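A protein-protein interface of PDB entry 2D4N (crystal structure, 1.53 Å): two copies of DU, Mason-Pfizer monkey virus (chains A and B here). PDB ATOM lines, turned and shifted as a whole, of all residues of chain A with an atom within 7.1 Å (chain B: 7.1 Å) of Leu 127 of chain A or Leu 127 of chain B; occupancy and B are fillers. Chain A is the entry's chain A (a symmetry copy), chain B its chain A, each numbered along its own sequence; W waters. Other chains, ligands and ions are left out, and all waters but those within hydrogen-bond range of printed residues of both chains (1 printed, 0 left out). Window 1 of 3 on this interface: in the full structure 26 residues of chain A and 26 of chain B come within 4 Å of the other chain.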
ATOM      1  N   LEU A  68     -15.698 -35.700 -27.403  1.00  0.00           N
ATOM      2  CA  LEU A  68     -15.768 -34.467 -28.148  1.00  0.00           C
ATOM      3  C   LEU A  68     -14.756 -33.469 -27.602  1.00  0.00           C
ATOM      4  O   LEU A  68     -14.124 -33.720 -26.550  1.00  0.00           O
ATOM      5  CB  LEU A  68     -17.163 -33.899 -28.014  1.00  0.00           C
ATOM      6  CG  LEU A  68     -18.097 -34.394 -29.129  1.00  0.00           C
ATOM      7  CD1 LEU A  68     -18.107 -35.824 -29.308  1.00  0.00           C
ATOM      8  CD2 LEU A  68     -19.493 -33.913 -28.796  1.00  0.00           C
ATOM      9  N   PRO A  69     -14.482 -32.415 -28.371  1.00  0.00           N
ATOM     10  CA  PRO A  69     -13.521 -31.411 -27.927  1.00  0.00           C
ATOM     11  C   PRO A  69     -13.908 -30.809 -26.578  1.00  0.00           C
ATOM     12  O   PRO A  69     -15.104 -30.716 -26.222  1.00  0.00           O
ATOM     13  CB  PRO A  69     -13.600 -30.335 -29.028  1.00  0.00           C
ATOM     14  CG  PRO A  69     -14.088 -31.045 -30.259  1.00  0.00           C
ATOM     15  CD  PRO A  69     -15.023 -32.138 -29.723  1.00  0.00           C
ATOM     16  N   PRO A  70     -12.911 -30.328 -25.825  1.00  0.00           N
ATOM     17  CA  PRO A  70     -13.209 -29.752 -24.529  1.00  0.00           C
ATOM     18  C   PRO A  70     -14.314 -28.678 -24.599  1.00  0.00           C
ATOM     19  O   PRO A  70     -14.341 -27.865 -25.530  1.00  0.00           O
ATOM     20  CB  PRO A  70     -11.854 -29.158 -24.090  1.00  0.00           C
ATOM     21  CG  PRO A  70     -10.840 -29.900 -24.876  1.00  0.00           C
ATOM     22  CD  PRO A  70     -11.462 -30.369 -26.103  1.00  0.00           C
ATOM     23  N   ASN A  71     -15.224 -28.697 -23.619  1.00  0.00           N
ATOM     24  CA  ASN A  71     -16.249 -27.645 -23.483  1.00  0.00           C
ATOM     25  C   ASN A  71     -17.294 -27.626 -24.603  1.00  0.00           C
ATOM     26  O   ASN A  71     -17.949 -26.616 -24.859  1.00  0.00           O
ATOM     27  CB  ASN A  71     -15.626 -26.269 -23.365  1.00  0.00           C
ATOM     28  CG  ASN A  71     -14.569 -26.222 -22.260  1.00  0.00           C
ATOM     29  OD1 ASN A  71     -14.820 -26.657 -21.138  1.00  0.00           O
ATOM     30  ND2 ASN A  71     -13.400 -25.761 -22.596  1.00  0.00           N
ATOM     31  N   THR A  72     -17.412 -28.771 -25.274  1.00  0.00           N
ATOM     32  CA  THR A  72     -18.446 -28.922 -26.321  1.00  0.00           C
ATOM     33  C   THR A  72     -19.259 -30.184 -26.134  1.00  0.00           C
ATOM     34  O   THR A  72     -18.826 -31.136 -25.482  1.00  0.00           O
ATOM     35  CB  THR A  72     -17.868 -29.015 -27.796  1.00  0.00           C
ATOM     36  OG1 THR A  72     -17.262 -30.298 -28.031  1.00  0.00           O
ATOM     37  CG2 THR A  72     -16.925 -27.870 -28.115  1.00  0.00           C
ATOM     38  N   PHE A  73     -20.472 -30.197 -26.713  1.00  0.00           N
ATOM     39  CA  PHE A  73     -21.242 -31.446 -26.800  1.00  0.00           C
ATOM     40  C   PHE A  73     -21.752 -31.502 -28.229  1.00  0.00           C
ATOM     41  O   PHE A  73     -21.496 -30.616 -29.033  1.00  0.00           O
ATOM     42  CB  PHE A  73     -22.389 -31.489 -25.760  1.00  0.00           C
ATOM     43  CG  PHE A  73     -23.552 -30.612 -26.095  1.00  0.00           C
ATOM     44  CD1 PHE A  73     -24.695 -31.173 -26.650  1.00  0.00           C
ATOM     45  CD2 PHE A  73     -23.519 -29.228 -25.828  1.00  0.00           C
ATOM     46  CE1 PHE A  73     -25.817 -30.366 -26.973  1.00  0.00           C
ATOM     47  CE2 PHE A  73     -24.658 -28.393 -26.153  1.00  0.00           C
ATOM     48  CZ  PHE A  73     -25.772 -28.990 -26.736  1.00  0.00           C
ATOM     49  N   GLY A  74     -22.438 -32.564 -28.588  1.00  0.00           N
ATOM     50  CA  GLY A  74     -22.840 -32.735 -29.999  1.00  0.00           C
ATOM     51  C   GLY A  74     -24.344 -32.925 -30.139  1.00  0.00           C
ATOM     52  O   GLY A  74     -25.015 -33.423 -29.206  1.00  0.00           O
ATOM     53  N   LEU A  75     -24.829 -32.604 -31.328  1.00  0.00           N
ATOM     54  CA  LEU A  75     -26.178 -33.023 -31.722  1.00  0.00           C
ATOM     55  C   LEU A  75     -26.038 -33.777 -33.048  1.00  0.00           C
ATOM     56  O   LEU A  75     -25.346 -33.333 -33.963  1.00  0.00           O
ATOM     57  CB  LEU A  75     -27.096 -31.818 -31.964  1.00  0.00           C
ATOM     58  CG  LEU A  75     -27.554 -30.992 -30.777  1.00  0.00           C
ATOM     59  CD1 LEU A  75     -28.515 -29.885 -31.253  1.00  0.00           C
ATOM     60  CD2 LEU A  75     -28.268 -31.865 -29.688  1.00  0.00           C
ATOM     61  N   ILE A 125     -23.295 -31.864 -35.265  1.00  0.00           N
ATOM     62  CA  ILE A 125     -23.015 -30.484 -35.016  1.00  0.00           C
ATOM     63  C   ILE A 125     -22.485 -30.299 -33.611  1.00  0.00           C
ATOM     64  O   ILE A 125     -22.920 -30.975 -32.668  1.00  0.00           O
ATOM     65  CB  ILE A 125     -24.263 -29.605 -35.283  1.00  0.00           C
ATOM     66  CG1 ILE A 125     -25.427 -30.133 -34.475  1.00  0.00           C
ATOM     67  CG2 ILE A 125     -24.594 -29.478 -36.833  1.00  0.00           C
ATOM     68  CD1 ILE A 125     -26.646 -29.228 -34.464  1.00  0.00           C
ATOM     69  N   LEU A 126     -21.486 -29.437 -33.457  1.00  0.00           N
ATOM     70  CA  LEU A 126     -20.826 -29.204 -32.136  1.00  0.00           C
ATOM     71  C   LEU A 126     -21.371 -27.917 -31.577  1.00  0.00           C
ATOM     72  O   LEU A 126     -21.515 -26.932 -32.303  1.00  0.00           O
ATOM     73  CB  LEU A 126     -19.310 -29.114 -32.296  1.00  0.00           C
ATOM     74  CG  LEU A 126     -18.658 -30.357 -32.878  1.00  0.00           C
ATOM     75  CD1 LEU A 126     -17.190 -30.036 -33.073  1.00  0.00           C
ATOM     76  CD2 LEU A 126     -18.838 -31.505 -31.860  1.00  0.00           C
ATOM     77  N   LEU A 127     -21.639 -27.941 -30.271  1.00  0.00           N
ATOM     78  CA  LEU A 127     -22.241 -26.817 -29.555  1.00  0.00           C
ATOM     79  C   LEU A 127     -21.519 -26.620 -28.226  1.00  0.00           C
ATOM     80  O   LEU A 127     -20.927 -27.586 -27.687  1.00  0.00           O
ATOM     81  CB  LEU A 127     -23.720 -27.086 -29.339  1.00  0.00           C
ATOM     82  CG  LEU A 127     -24.489 -27.015 -30.678  1.00  0.00           C
ATOM     83  CD1 LEU A 127     -25.913 -27.427 -30.417  1.00  0.00           C
ATOM     84  CD2 LEU A 127     -24.483 -25.599 -31.271  1.00  0.00           C
ATOM     85  N   PRO A 128     -21.484 -25.358 -27.730  1.00  0.00           N
ATOM     86  CA  PRO A 128     -20.843 -25.078 -26.444  1.00  0.00           C
ATOM     87  C   PRO A 128     -21.606 -25.743 -25.302  1.00  0.00           C
ATOM     88  O   PRO A 128     -22.852 -25.832 -25.321  1.00  0.00           O
ATOM     89  CB  PRO A 128     -20.913 -23.561 -26.344  1.00  0.00           C
ATOM     90  CG  PRO A 128     -22.047 -23.153 -27.215  1.00  0.00           C
ATOM     91  CD  PRO A 128     -22.043 -24.135 -28.360  1.00  0.00           C
ATOM     92  N   LEU A 129     -20.854 -26.302 -24.374  1.00  0.00           N
ATOM     93  CA  LEU A 129     -21.465 -26.937 -23.228  1.00  0.00           C
ATOM     94  C   LEU A 129     -21.515 -25.938 -22.084  1.00  0.00           C
ATOM     95  O   LEU A 129     -20.469 -25.509 -21.584  1.00  0.00           O
ATOM     96  CB  LEU A 129     -20.649 -28.175 -22.867  1.00  0.00           C
ATOM     97  CG  LEU A 129     -21.110 -28.982 -21.632  1.00  0.00           C
ATOM     98  CD1 LEU A 129     -22.539 -29.541 -21.788  1.00  0.00           C
ATOM     99  CD2 LEU A 129     -20.117 -30.165 -21.394  1.00  0.00           C
ATOM    100  N   ILE A 130     -22.730 -25.576 -21.682  1.00  0.00           N
ATOM    101  CA  ILE A 130     -22.879 -24.624 -20.625  1.00  0.00           C
ATOM    102  C   ILE A 130     -22.839 -25.362 -19.285  1.00  0.00           C
ATOM    103  O   ILE A 130     -23.463 -26.423 -19.111  1.00  0.00           O
ATOM    104  CB  ILE A 130     -24.188 -23.873 -20.823  1.00  0.00           C
ATOM    105  CG1 ILE A 130     -24.057 -22.976 -22.053  1.00  0.00           C
ATOM    106  CG2 ILE A 130     -24.545 -23.083 -19.585  1.00  0.00           C
ATOM    107  CD1 ILE A 130     -25.274 -22.248 -22.422  1.00  0.00           C
ATOM    108  N   LEU B  68     -35.064 -19.496 -17.720  1.00  0.00           N
ATOM    109  CA  LEU B  68     -33.751 -20.070 -17.888  1.00  0.00           C
ATOM    110  C   LEU B  68     -32.686 -19.071 -17.459  1.00  0.00           C
ATOM    111  O   LEU B  68     -33.000 -17.892 -17.177  1.00  0.00           O
ATOM    112  CB  LEU B  68     -33.561 -20.420 -19.347  1.00  0.00           C
ATOM    113  CG  LEU B  68     -34.009 -21.856 -19.660  1.00  0.00           C
ATOM    114  CD1 LEU B  68     -35.334 -22.181 -19.191  1.00  0.00           C
ATOM    115  CD2 LEU B  68     -33.943 -22.033 -21.162  1.00  0.00           C
ATOM    116  N   PRO B  69     -31.460 -19.556 -17.259  1.00  0.00           N
ATOM    117  CA  PRO B  69     -30.379 -18.669 -16.842  1.00  0.00           C
ATOM    118  C   PRO B  69     -30.179 -17.514 -17.821  1.00  0.00           C
ATOM    119  O   PRO B  69     -30.439 -17.636 -19.040  1.00  0.00           O
ATOM    120  CB  PRO B  69     -29.142 -19.590 -16.852  1.00  0.00           C
ATOM    121  CG  PRO B  69     -29.671 -20.984 -16.664  1.00  0.00           C
ATOM    122  CD  PRO B  69     -31.036 -20.973 -17.365  1.00  0.00           C
ATOM    123  N   PRO B  70     -29.651 -16.388 -17.324  1.00  0.00           N
ATOM    124  CA  PRO B  70     -29.444 -15.251 -18.198  1.00  0.00           C
ATOM    125  C   PRO B  70     -28.662 -15.621 -19.476  1.00  0.00           C
ATOM    126  O   PRO B  70     -27.700 -16.395 -19.420  1.00  0.00           O
ATOM    127  CB  PRO B  70     -28.662 -14.262 -17.308  1.00  0.00           C
ATOM    128  CG  PRO B  70     -28.969 -14.677 -15.919  1.00  0.00           C
ATOM    129  CD  PRO B  70     -29.300 -16.092 -15.921  1.00  0.00           C
ATOM    130  N   ASN B  71     -29.095 -15.073 -20.616  1.00  0.00           N
ATOM    131  CA  ASN B  71     -28.358 -15.226 -21.885  1.00  0.00           C
ATOM    132  C   ASN B  71     -28.344 -16.653 -22.446  1.00  0.00           C
ATOM    133  O   ASN B  71     -27.481 -17.027 -23.239  1.00  0.00           O
ATOM    134  CB  ASN B  71     -26.933 -14.727 -21.769  1.00  0.00           C
ATOM    135  CG  ASN B  71     -26.878 -13.303 -21.212  1.00  0.00           C
ATOM    136  OD1 ASN B  71     -27.584 -12.419 -21.691  1.00  0.00           O
ATOM    137  ND2 ASN B  71     -26.101 -13.112 -20.187  1.00  0.00           N
ATOM    138  N   THR B  72     -29.319 -17.438 -21.991  1.00  0.00           N
ATOM    139  CA  THR B  72     -29.479 -18.812 -22.516  1.00  0.00           C
ATOM    140  C   THR B  72     -30.904 -19.091 -22.940  1.00  0.00           C
ATOM    141  O   THR B  72     -31.847 -18.433 -22.498  1.00  0.00           O
ATOM    142  CB  THR B  72     -29.126 -19.952 -21.472  1.00  0.00           C
ATOM    143  OG1 THR B  72     -30.156 -20.077 -20.477  1.00  0.00           O
ATOM    144  CG2 THR B  72     -27.753 -19.757 -20.853  1.00  0.00           C
ATOM    145  N   PHE B  73     -31.073 -20.089 -23.825  1.00  0.00           N
ATOM    146  CA  PHE B  73     -32.419 -20.602 -24.121  1.00  0.00           C
ATOM    147  C   PHE B  73     -32.288 -22.114 -24.076  1.00  0.00           C
ATOM    148  O   PHE B  73     -31.218 -22.655 -23.832  1.00  0.00           O
ATOM    149  CB  PHE B  73     -32.941 -20.093 -25.488  1.00  0.00           C
ATOM    150  CG  PHE B  73     -32.303 -20.750 -26.669  1.00  0.00           C
ATOM    151  CD1 PHE B  73     -32.982 -21.760 -27.341  1.00  0.00           C
ATOM    152  CD2 PHE B  73     -31.036 -20.340 -27.133  1.00  0.00           C
ATOM    153  CE1 PHE B  73     -32.405 -22.397 -28.469  1.00  0.00           C
ATOM    154  CE2 PHE B  73     -30.436 -20.983 -28.284  1.00  0.00           C
ATOM    155  CZ  PHE B  73     -31.136 -22.011 -28.909  1.00  0.00           C
ATOM    156  N   GLY B  74     -33.379 -22.823 -24.260  1.00  0.00           N
ATOM    157  CA  GLY B  74     -33.338 -24.290 -24.090  1.00  0.00           C
ATOM    158  C   GLY B  74     -33.834 -25.016 -25.333  1.00  0.00           C
ATOM    159  O   GLY B  74     -34.658 -24.473 -26.105  1.00  0.00           O
ATOM    160  N   LEU B  75     -33.390 -26.257 -25.456  1.00  0.00           N
ATOM    161  CA  LEU B  75     -34.014 -27.183 -26.408  1.00  0.00           C
ATOM    162  C   LEU B  75     -34.420 -28.427 -25.613  1.00  0.00           C
ATOM    163  O   LEU B  75     -33.648 -28.952 -24.812  1.00  0.00           O
ATOM    164  CB  LEU B  75     -33.029 -27.624 -27.497  1.00  0.00           C
ATOM    165  CG  LEU B  75     -32.598 -26.621 -28.550  1.00  0.00           C
ATOM    166  CD1 LEU B  75     -31.667 -27.304 -29.569  1.00  0.00           C
ATOM    167  CD2 LEU B  75     -33.821 -25.992 -29.304  1.00  0.00           C
ATOM    168  N   ILE B 125     -31.508 -29.197 -22.964  1.00  0.00           N
ATOM    169  CA  ILE B 125     -30.184 -28.709 -23.199  1.00  0.00           C
ATOM    170  C   ILE B 125     -30.182 -27.197 -23.256  1.00  0.00           C
ATOM    171  O   ILE B 125     -31.123 -26.574 -23.767  1.00  0.00           O
ATOM    172  CB  ILE B 125     -29.579 -29.336 -24.480  1.00  0.00           C
ATOM    173  CG1 ILE B 125     -30.517 -29.100 -25.642  1.00  0.00           C
ATOM    174  CG2 ILE B 125     -29.209 -30.870 -24.286  1.00  0.00           C
ATOM    175  CD1 ILE B 125     -29.939 -29.457 -26.999  1.00  0.00           C
ATOM    176  N   LEU B 126     -29.166 -26.578 -22.664  1.00  0.00           N
ATOM    177  CA  LEU B 126     -29.071 -25.087 -22.590  1.00  0.00           C
ATOM    178  C   LEU B 126     -28.090 -24.642 -23.641  1.00  0.00           C
ATOM    179  O   LEU B 126     -27.034 -25.255 -23.811  1.00  0.00           O
ATOM    180  CB  LEU B 126     -28.604 -24.643 -21.206  1.00  0.00           C
ATOM    181  CG  LEU B 126     -29.514 -25.063 -20.063  1.00  0.00           C
ATOM    182  CD1 LEU B 126     -28.831 -24.644 -18.778  1.00  0.00           C
ATOM    183  CD2 LEU B 126     -30.860 -24.326 -20.235  1.00  0.00           C
ATOM    184  N   LEU B 127     -28.449 -23.551 -24.317  1.00  0.00           N
ATOM    185  CA  LEU B 127     -27.669 -23.001 -25.426  1.00  0.00           C
ATOM    186  C   LEU B 127     -27.596 -21.484 -25.289  1.00  0.00           C
ATOM    187  O   LEU B 127     -28.491 -20.869 -24.661  1.00  0.00           O
ATOM    188  CB  LEU B 127     -28.309 -23.401 -26.745  1.00  0.00           C
ATOM    189  CG  LEU B 127     -28.136 -24.916 -26.998  1.00  0.00           C
ATOM    190  CD1 LEU B 127     -28.909 -25.267 -28.241  1.00  0.00           C
ATOM    191  CD2 LEU B 127     -26.666 -25.300 -27.203  1.00  0.00           C
ATOM    192  N   PRO B 128     -26.493 -20.877 -25.792  1.00  0.00           N
ATOM    193  CA  PRO B 128     -26.350 -19.421 -25.737  1.00  0.00           C
ATOM    194  C   PRO B 128     -27.396 -18.740 -26.614  1.00  0.00           C
ATOM    195  O   PRO B 128     -27.763 -19.244 -27.696  1.00  0.00           O
ATOM    196  CB  PRO B 128     -24.944 -19.189 -26.274  1.00  0.00           C
ATOM    197  CG  PRO B 128     -24.634 -20.377 -27.112  1.00  0.00           C
ATOM    198  CD  PRO B 128     -25.326 -21.534 -26.435  1.00  0.00           C
ATOM    199  N   LEU B 129     -27.951 -17.662 -26.093  1.00  0.00           N
ATOM    200  CA  LEU B 129     -28.934 -16.916 -26.845  1.00  0.00           C
ATOM    201  C   LEU B 129     -28.237 -15.776 -27.568  1.00  0.00           C
ATOM    202  O   LEU B 129     -27.695 -14.869 -26.926  1.00  0.00           O
ATOM    203  CB  LEU B 129     -30.000 -16.407 -25.877  1.00  0.00           C
ATOM    204  CG  LEU B 129     -31.133 -15.542 -26.473  1.00  0.00           C
ATOM    205  CD1 LEU B 129     -31.958 -16.294 -27.537  1.00  0.00           C
ATOM    206  CD2 LEU B 129     -32.079 -15.072 -25.323  1.00  0.00           C
ATOM    207  N   ILE B 130     -28.256 -15.833 -28.897  1.00  0.00           N
ATOM    208  CA  ILE B 130     -27.607 -14.817 -29.666  1.00  0.00           C
ATOM    209  C   ILE B 130     -28.581 -13.654 -29.869  1.00  0.00           C
ATOM    210  O   ILE B 130     -29.769 -13.851 -30.178  1.00  0.00           O
ATOM    211  CB  ILE B 130     -27.152 -15.417 -30.988  1.00  0.00           C
ATOM    212  CG1 ILE B 130     -26.011 -16.396 -30.713  1.00  0.00           C
ATOM    213  CG2 ILE B 130     -26.743 -14.332 -31.956  1.00  0.00           C
ATOM    214  CD1 ILE B 130     -25.521 -17.121 -31.889  1.00  0.00           C
HETATM  215  O   HOH W   1     -24.874 -26.662 -23.235  1.00  0.00           O
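OG1 of Thr 72 of chain B sits at hydrogen-bond distance from O of Pro 69 of chain B.
The backbone NH (N) of Phe 73 of chain B lies within hydrogen-bond range of the backbone carbonyl oxygen (O) of Leu 127 of chain B, at 2.8 Å.
O of Leu 75 of chain B sits at hydrogen-bond distance from N of Ile 125 of chain B.
The backbone carbonyl oxygen of Leu 127 of chain A is in hydrogen-bond range of the backbone NH of Phe 73 of chain A.
The backbone carbonyl oxygen (O) of Leu 75 of chain A is in hydrogen-bond range of the backbone NH (N) of Ile 125 of chain A (2.8 Å).
CZ of Phe 73 of chain A touches CD2 of Leu 127 of chain B, 3.8 Å away.
CD2 of Leu 75 of chain A touches CD1 of Ile 125 of chain B, 3.98 Å away.
Leu 127 of chain A touches Leu 127 of chain B (CD1 to CD2, 3.9 Å).
Pro 128 of chain B touches Pro 128 of chain A.
Thr 72 of chain B touches Ile 130 of chain A (CG2 to CD1, 3.8 Å).
Leu 126 of chain B touches Ile 130 of chain A (O to CD1, 3.8 Å).
CD1 of Ile 130 of chain A touches C of Leu 127 of chain B (3.8 Å).
Pro 128 of chain B touches Ile 130 of chain A (N to CD1, 3.8 Å).
Of the printed residues of chain B, Leu 75 of chain A touches Ile 125 (3.98 Å).
Printed residues of chain A within 4 Å of Thr 72 of chain B: Ile 130 (3.8 Å).
Printed residues of chain B within 4 Å of Phe 73 of chain A: Leu 127.
Printed residues of chain A within 4 Å of Leu 126 of chain B: Ile 130.
The nearest printed residue of chain B that does not touch Leu 127 of chain A is Ile 125 of chain B (5.7 Å).
Hydrophobic or aromatic side chains of chain B within 4 Å of the printed part of chain A: Ile 125, Leu 127 and Pro 128.
Phe 73 of chain A touches Leu 127 of chain B, but with the chains exchanged Leu 127 of chain A does not touch Phe 73 of chain B (7.7 Å).
Ile 130 of chain A touches Leu 126 of chain B, but with the chains exchanged Leu 126 of chain A does not touch Ile 130 of chain B (10.6 Å).
Ile 130 of chain A touches Leu 127 of chain B, but with the chains exchanged Leu 127 of chain A does not touch Ile 130 of chain B (8.6 Å).
Ile 130 of chain A touches Pro 128 of chain B, but with the chains exchanged Pro 128 of chain A does not touch Ile 130 of chain B (8.4 Å).
Positions printed for both chains: 68, 69, 70, 71, 72, 73, 74, 75, 125, 126, 127, 128, 129 and 130.
Of the 8 pairs that touch across the chains among the printed residues, 2 have their exchanged pair printed and touching as well.
Water W1 lies within hydrogen-bond range of the backbone carbonyl oxygen of Leu 126 of chain B (2.6 Å), the backbone NH of Ile 130 of chain A (2.9 Å) and the backbone carbonyl oxygen of Pro 128 of chain A (3.0 Å).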
